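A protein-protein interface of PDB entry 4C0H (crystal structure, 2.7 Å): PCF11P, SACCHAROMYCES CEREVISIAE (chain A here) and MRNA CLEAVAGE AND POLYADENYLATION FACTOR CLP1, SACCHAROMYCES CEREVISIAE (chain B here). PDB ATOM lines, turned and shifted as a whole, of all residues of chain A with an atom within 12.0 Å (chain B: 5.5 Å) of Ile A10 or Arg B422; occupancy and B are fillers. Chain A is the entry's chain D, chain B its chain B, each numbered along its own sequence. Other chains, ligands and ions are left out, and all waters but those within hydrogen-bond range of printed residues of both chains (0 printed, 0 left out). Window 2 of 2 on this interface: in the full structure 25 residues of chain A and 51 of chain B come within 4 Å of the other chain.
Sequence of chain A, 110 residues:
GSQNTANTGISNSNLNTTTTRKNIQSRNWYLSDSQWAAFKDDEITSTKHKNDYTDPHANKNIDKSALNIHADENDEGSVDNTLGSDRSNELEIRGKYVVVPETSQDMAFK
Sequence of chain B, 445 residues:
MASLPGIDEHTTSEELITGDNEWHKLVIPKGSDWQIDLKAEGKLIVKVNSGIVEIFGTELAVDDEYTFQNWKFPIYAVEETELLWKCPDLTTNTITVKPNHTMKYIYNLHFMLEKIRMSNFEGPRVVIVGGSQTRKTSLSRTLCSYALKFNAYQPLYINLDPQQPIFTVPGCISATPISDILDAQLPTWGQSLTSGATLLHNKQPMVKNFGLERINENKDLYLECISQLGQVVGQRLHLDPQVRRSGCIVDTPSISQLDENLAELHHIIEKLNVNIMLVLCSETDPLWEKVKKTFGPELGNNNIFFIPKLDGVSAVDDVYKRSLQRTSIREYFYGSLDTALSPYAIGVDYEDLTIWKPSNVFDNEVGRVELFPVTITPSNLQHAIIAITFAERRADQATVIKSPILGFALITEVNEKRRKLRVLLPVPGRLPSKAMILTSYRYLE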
ATOM      1  N   GLY A   9      24.775 -19.850 -23.675  1.00  0.00           N
ATOM      2  CA  GLY A   9      25.002 -21.232 -24.092  1.00  0.00           C
ATOM      3  C   GLY A   9      26.330 -21.500 -24.783  1.00  0.00           C
ATOM      4  O   GLY A   9      27.357 -20.944 -24.382  1.00  0.00           O
ATOM      5  N   ILE A  10      26.323 -22.385 -25.827  1.00  0.00           N
ATOM      6  CA  ILE A  10      27.499 -22.745 -26.650  1.00  0.00           C
ATOM      7  C   ILE A  10      27.227 -22.739 -28.202  1.00  0.00           C
ATOM      8  O   ILE A  10      26.059 -22.623 -28.601  1.00  0.00           O
ATOM      9  CB  ILE A  10      28.243 -23.996 -26.100  1.00  0.00           C
ATOM     10  CG1 ILE A  10      29.776 -23.857 -26.232  1.00  0.00           C
ATOM     11  CG2 ILE A  10      27.717 -25.306 -26.684  1.00  0.00           C
ATOM     12  CD1 ILE A  10      30.472 -22.942 -25.143  1.00  0.00           C
ATOM     13  N   SER A  11      28.306 -22.833 -29.052  1.00  0.00           N
ATOM     14  CA  SER A  11      28.321 -22.814 -30.542  1.00  0.00           C
ATOM     15  C   SER A  11      27.071 -23.245 -31.350  1.00  0.00           C
ATOM     16  O   SER A  11      26.891 -24.433 -31.611  1.00  0.00           O
ATOM     17  CB  SER A  11      29.584 -23.488 -31.090  1.00  0.00           C
ATOM     18  OG  SER A  11      29.510 -23.807 -32.475  1.00  0.00           O
ATOM     19  N   ASN A  12      26.263 -22.263 -31.811  1.00  0.00           N
ATOM     20  CA  ASN A  12      25.087 -22.507 -32.657  1.00  0.00           C
ATOM     21  C   ASN A  12      25.534 -22.734 -34.134  1.00  0.00           C
ATOM     22  O   ASN A  12      26.707 -22.491 -34.454  1.00  0.00           O
ATOM     23  CB  ASN A  12      24.035 -21.404 -32.491  1.00  0.00           C
ATOM     24  CG  ASN A  12      22.965 -21.648 -31.428  1.00  0.00           C
ATOM     25  OD1 ASN A  12      23.085 -22.452 -30.494  1.00  0.00           O
ATOM     26  ND2 ASN A  12      21.878 -20.917 -31.543  1.00  0.00           N
ATOM     27  N   SER A  13      24.644 -23.290 -34.955  1.00  0.00           N
ATOM     28  CA  SER A  13      24.909 -23.775 -36.311  1.00  0.00           C
ATOM     29  C   SER A  13      25.532 -25.161 -36.469  1.00  0.00           C
ATOM     30  O   SER A  13      25.541 -25.958 -35.572  1.00  0.00           O
ATOM     31  CB  SER A  13      25.731 -22.774 -37.091  1.00  0.00           C
ATOM     32  OG  SER A  13      26.180 -23.308 -38.332  1.00  0.00           O
ATOM     33  N   ASN A  14      26.038 -25.420 -37.661  1.00  0.00           N
ATOM     34  CA  ASN A  14      26.718 -26.663 -38.003  1.00  0.00           C
ATOM     35  C   ASN A  14      27.799 -27.027 -36.987  1.00  0.00           C
ATOM     36  O   ASN A  14      28.635 -26.181 -36.620  1.00  0.00           O
ATOM     37  CB  ASN A  14      27.332 -26.585 -39.407  1.00  0.00           C
ATOM     38  CG  ASN A  14      26.324 -26.629 -40.505  1.00  0.00           C
ATOM     39  OD1 ASN A  14      25.815 -27.707 -40.870  1.00  0.00           O
ATOM     40  ND2 ASN A  14      26.041 -25.453 -41.075  1.00  0.00           N
ATOM     41  N   LEU A  15      27.783 -28.296 -36.547  1.00  0.00           N
ATOM     42  CA  LEU A  15      28.771 -28.767 -35.601  1.00  0.00           C
ATOM     43  C   LEU A  15      29.738 -29.742 -36.281  1.00  0.00           C
ATOM     44  O   LEU A  15      29.469 -30.181 -37.400  1.00  0.00           O
ATOM     45  CB  LEU A  15      28.087 -29.378 -34.374  1.00  0.00           C
ATOM     46  CG  LEU A  15      27.222 -28.488 -33.454  1.00  0.00           C
ATOM     47  CD1 LEU A  15      27.141 -29.103 -32.076  1.00  0.00           C
ATOM     48  CD2 LEU A  15      27.759 -27.066 -33.298  1.00  0.00           C
ATOM     49  N   ASN A  16      30.876 -30.053 -35.621  1.00  0.00           N
ATOM     50  CA  ASN A  16      31.932 -30.954 -36.101  1.00  0.00           C
ATOM     51  C   ASN A  16      32.173 -32.088 -35.102  1.00  0.00           C
ATOM     52  O   ASN A  16      32.999 -32.969 -35.340  1.00  0.00           O
ATOM     53  CB  ASN A  16      33.226 -30.169 -36.331  1.00  0.00           C
ATOM     54  CG  ASN A  16      33.118 -29.105 -37.398  1.00  0.00           C
ATOM     55  OD1 ASN A  16      33.057 -29.400 -38.600  1.00  0.00           O
ATOM     56  ND2 ASN A  16      33.112 -27.844 -36.982  1.00  0.00           N
ATOM     57  N   ALA B 345      22.778 -26.935 -34.643  1.00  0.00           N
ATOM     58  CA  ALA B 345      22.330 -26.407 -33.364  1.00  0.00           C
ATOM     59  C   ALA B 345      21.541 -25.119 -33.533  1.00  0.00           C
ATOM     60  O   ALA B 345      21.932 -24.178 -34.243  1.00  0.00           O
ATOM     61  CB  ALA B 345      23.522 -26.175 -32.450  1.00  0.00           C
ATOM     62  N   ILE B 346      20.433 -25.060 -32.825  1.00  0.00           N
ATOM     63  CA  ILE B 346      19.546 -23.917 -32.891  1.00  0.00           C
ATOM     64  C   ILE B 346      19.113 -23.539 -31.493  1.00  0.00           C
ATOM     65  O   ILE B 346      19.029 -24.398 -30.606  1.00  0.00           O
ATOM     66  CB  ILE B 346      18.314 -24.223 -33.811  1.00  0.00           C
ATOM     67  CG1 ILE B 346      17.543 -25.465 -33.352  1.00  0.00           C
ATOM     68  CG2 ILE B 346      18.701 -24.368 -35.283  1.00  0.00           C
ATOM     69  CD1 ILE B 346      16.128 -25.425 -33.711  1.00  0.00           C
ATOM     70  N   GLY B 347      18.832 -22.254 -31.322  1.00  0.00           N
ATOM     71  CA  GLY B 347      18.293 -21.701 -30.093  1.00  0.00           C
ATOM     72  C   GLY B 347      16.815 -21.428 -30.292  1.00  0.00           C
ATOM     73  O   GLY B 347      16.433 -20.805 -31.288  1.00  0.00           O
ATOM     74  N   VAL B 348      15.960 -21.924 -29.378  1.00  0.00           N
ATOM     75  CA  VAL B 348      14.504 -21.725 -29.465  1.00  0.00           C
ATOM     76  C   VAL B 348      13.883 -21.268 -28.145  1.00  0.00           C
ATOM     77  O   VAL B 348      14.390 -21.603 -27.077  1.00  0.00           O
ATOM     78  CB  VAL B 348      13.736 -22.937 -30.068  1.00  0.00           C
ATOM     79  CG1 VAL B 348      14.071 -23.131 -31.541  1.00  0.00           C
ATOM     80  CG2 VAL B 348      13.985 -24.211 -29.282  1.00  0.00           C
ATOM     81  N   LEU B 410      18.001 -33.511 -29.958  1.00  0.00           N
ATOM     82  CA  LEU B 410      18.611 -33.533 -28.638  1.00  0.00           C
ATOM     83  C   LEU B 410      18.552 -32.140 -28.031  1.00  0.00           C
ATOM     84  O   LEU B 410      18.999 -31.175 -28.660  1.00  0.00           O
ATOM     85  CB  LEU B 410      20.055 -34.045 -28.710  1.00  0.00           C
ATOM     86  CG  LEU B 410      20.910 -33.930 -27.442  1.00  0.00           C
ATOM     87  CD1 LEU B 410      20.526 -34.983 -26.410  1.00  0.00           C
ATOM     88  CD2 LEU B 410      22.390 -34.049 -27.780  1.00  0.00           C
ATOM     89  N   ILE B 411      17.966 -32.032 -26.823  1.00  0.00           N
ATOM     90  CA  ILE B 411      17.912 -30.759 -26.100  1.00  0.00           C
ATOM     91  C   ILE B 411      19.148 -30.705 -25.201  1.00  0.00           C
ATOM     92  O   ILE B 411      19.219 -31.351 -24.162  1.00  0.00           O
ATOM     93  CB  ILE B 411      16.566 -30.550 -25.361  1.00  0.00           C
ATOM     94  CG1 ILE B 411      15.378 -30.585 -26.370  1.00  0.00           C
ATOM     95  CG2 ILE B 411      16.582 -29.247 -24.530  1.00  0.00           C
ATOM     96  CD1 ILE B 411      14.018 -30.542 -25.753  1.00  0.00           C
ATOM     97  N   THR B 412      20.124 -29.946 -25.662  1.00  0.00           N
ATOM     98  CA  THR B 412      21.461 -29.727 -25.139  1.00  0.00           C
ATOM     99  C   THR B 412      21.540 -28.919 -23.856  1.00  0.00           C
ATOM    100  O   THR B 412      22.389 -29.174 -22.996  1.00  0.00           O
ATOM    101  CB  THR B 412      22.242 -29.092 -26.292  1.00  0.00           C
ATOM    102  OG1 THR B 412      22.549 -30.156 -27.208  1.00  0.00           O
ATOM    103  CG2 THR B 412      23.509 -28.361 -25.850  1.00  0.00           C
ATOM    104  N   GLU B 413      20.705 -27.893 -23.775  1.00  0.00           N
ATOM    105  CA  GLU B 413      20.721 -26.910 -22.710  1.00  0.00           C
ATOM    106  C   GLU B 413      19.347 -26.294 -22.532  1.00  0.00           C
ATOM    107  O   GLU B 413      18.633 -26.073 -23.510  1.00  0.00           O
ATOM    108  CB  GLU B 413      21.729 -25.814 -23.087  1.00  0.00           C
ATOM    109  CG  GLU B 413      22.379 -25.125 -21.906  1.00  0.00           C
ATOM    110  CD  GLU B 413      23.279 -23.972 -22.310  1.00  0.00           C
ATOM    111  OE1 GLU B 413      24.382 -24.237 -22.843  1.00  0.00           O
ATOM    112  OE2 GLU B 413      22.883 -22.805 -22.080  1.00  0.00           O
ATOM    113  N   VAL B 414      18.969 -26.035 -21.274  1.00  0.00           N
ATOM    114  CA  VAL B 414      17.702 -25.390 -20.925  1.00  0.00           C
ATOM    115  C   VAL B 414      18.046 -24.215 -20.029  1.00  0.00           C
ATOM    116  O   VAL B 414      18.603 -24.415 -18.951  1.00  0.00           O
ATOM    117  CB  VAL B 414      16.635 -26.340 -20.291  1.00  0.00           C
ATOM    118  CG1 VAL B 414      15.376 -25.568 -19.885  1.00  0.00           C
ATOM    119  CG2 VAL B 414      16.269 -27.486 -21.236  1.00  0.00           C
ATOM    120  N   LYS B 420      14.851 -19.972 -22.929  1.00  0.00           N
ATOM    121  CA  LYS B 420      15.358 -20.529 -24.173  1.00  0.00           C
ATOM    122  C   LYS B 420      15.989 -21.913 -24.032  1.00  0.00           C
ATOM    123  O   LYS B 420      16.388 -22.317 -22.940  1.00  0.00           O
ATOM    124  CB  LYS B 420      16.310 -19.533 -24.873  1.00  0.00           C
ATOM    125  CG  LYS B 420      15.599 -18.273 -25.402  1.00  0.00           C
ATOM    126  CD  LYS B 420      16.465 -17.409 -26.300  1.00  0.00           C
ATOM    127  CE  LYS B 420      16.372 -15.922 -25.970  1.00  0.00           C
ATOM    128  NZ  LYS B 420      15.154 -15.238 -26.513  1.00  0.00           N
ATOM    129  N   LEU B 421      16.053 -22.646 -25.151  1.00  0.00           N
ATOM    130  CA  LEU B 421      16.618 -23.991 -25.222  1.00  0.00           C
ATOM    131  C   LEU B 421      17.590 -24.082 -26.390  1.00  0.00           C
ATOM    132  O   LEU B 421      17.341 -23.494 -27.449  1.00  0.00           O
ATOM    133  CB  LEU B 421      15.519 -25.072 -25.442  1.00  0.00           C
ATOM    134  CG  LEU B 421      14.370 -25.182 -24.455  1.00  0.00           C
ATOM    135  CD1 LEU B 421      13.191 -24.367 -24.925  1.00  0.00           C
ATOM    136  CD2 LEU B 421      13.899 -26.612 -24.333  1.00  0.00           C
ATOM    137  N   ARG B 422      18.670 -24.857 -26.211  1.00  0.00           N
ATOM    138  CA  ARG B 422      19.599 -25.163 -27.286  1.00  0.00           C
ATOM    139  C   ARG B 422      19.204 -26.580 -27.761  1.00  0.00           C
ATOM    140  O   ARG B 422      19.216 -27.541 -26.973  1.00  0.00           O
ATOM    141  CB  ARG B 422      21.081 -25.082 -26.852  1.00  0.00           C
ATOM    142  CG  ARG B 422      22.003 -24.671 -28.018  1.00  0.00           C
ATOM    143  CD  ARG B 422      23.495 -24.934 -27.837  1.00  0.00           C
ATOM    144  NE  ARG B 422      23.898 -26.330 -28.100  1.00  0.00           N
ATOM    145  CZ  ARG B 422      24.874 -26.719 -28.916  1.00  0.00           C
ATOM    146  NH1 ARG B 422      25.524 -25.834 -29.656  1.00  0.00           N
ATOM    147  NH2 ARG B 422      25.152 -28.009 -29.061  1.00  0.00           N
ATOM    148  N   VAL B 423      18.775 -26.684 -29.030  1.00  0.00           N
ATOM    149  CA  VAL B 423      18.337 -27.939 -29.642  1.00  0.00           C
ATOM    150  C   VAL B 423      19.302 -28.328 -30.771  1.00  0.00           C
ATOM    151  O   VAL B 423      19.682 -27.495 -31.603  1.00  0.00           O
ATOM    152  CB  VAL B 423      16.865 -27.840 -30.143  1.00  0.00           C
ATOM    153  CG1 VAL B 423      16.346 -29.183 -30.651  1.00  0.00           C
ATOM    154  CG2 VAL B 423      15.948 -27.305 -29.049  1.00  0.00           C
ATOM    155  N   LEU B 424      19.702 -29.601 -30.784  1.00  0.00           N
ATOM    156  CA  LEU B 424      20.558 -30.145 -31.832  1.00  0.00           C
ATOM    157  C   LEU B 424      19.670 -30.958 -32.770  1.00  0.00           C
ATOM    158  O   LEU B 424      18.924 -31.830 -32.312  1.00  0.00           O
ATOM    159  CB  LEU B 424      21.705 -31.001 -31.245  1.00  0.00           C
ATOM    160  CG  LEU B 424      22.764 -31.481 -32.243  1.00  0.00           C
ATOM    161  CD1 LEU B 424      23.725 -30.333 -32.634  1.00  0.00           C
ATOM    162  CD2 LEU B 424      23.503 -32.712 -31.704  1.00  0.00           C
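Hydrophobic or aromatic side chains of chain A that line the printed part of chain B: Ile A10 and Leu A15.
Among the printed residues, merely in contact across the chains: Gly A9 with Glu B413 (3.3 Å), Ser A11 with Ala B345 (3.9 Å), Asn A12 with Ala B345 (3.9 Å), Asn A12 with Ile B346 (3.8 Å), Asn A12 with Arg B422 (3.5 Å), Leu A15 with Arg B422 (3.8 Å) and Leu A15 with Leu B424 (3.7 Å).
O of Ala B345 is in hydrogen-bond range of N of Ser A13 (2.9 Å). N of Gly B347 sits close to ND2 of Asn A12, 3.3 Å away. NH1 of Arg B422 is in hydrogen-bond range of O of Ile A10. NH1 of Arg B422 is in hydrogen-bond range of O of Ser A11 (2.8 Å).
The backbone carbonyl oxygen (O) of Ile B346 sits at hydrogen-bond distance from the backbone NH (N) of Val B423, at 2.8 Å. O of Leu B410 is in hydrogen-bond range of N of Leu B424 (2.7 Å). O of Arg B422 is in hydrogen-bond range of N of Thr B412, 2.9 Å away. The backbone carbonyl oxygen (O) of Glu B413 lies within hydrogen-bond range of the backbone NH (N) of Arg B422 (3.0 Å). The side-chain amide nitrogen (ND2) of Asn A14 sits close to the side-chain hydroxyl (OG) of Ser A13 (3.5 Å).
Of the printed residues of chain B, Ile A10 touches Arg B422. Printed residues of chain B within 4 Å of Ser A11: Ala B345 (3.9 Å) and Arg B422 (2.8 Å). Printed residues of chain B within 4 Å of Ser A13: Ala B345 (2.9 Å). Of chain A, only Asn A12 (3.8 Å) comes within 4 Å of Ile B346. Gly B347 touches just one residue of chain A: Asn A12 (3.3 Å). No residue of chain A comes within 4 Å of Val B348. No residue of chain A comes within 4 Å of Leu B410. No residue of chain A comes within 4 Å of Thr B412. Of chain A, only Ile A10, Ser A11, Asn A12 and Leu A15 come within 4 Å of Arg B422. No residue of chain A comes within 4 Å of Val B423. Leu B424 touches just one residue of chain A: Leu A15. The nearest printed residue of chain B that does not touch Ile A10 is Glu B413 (4.01 Å). The nearest residue of chain A that does not touch Arg B422 is Gly A9 (5.4 Å). The nearest printed residue of chain B that does not touch Leu A15 is Ala B345 (4.4 Å).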
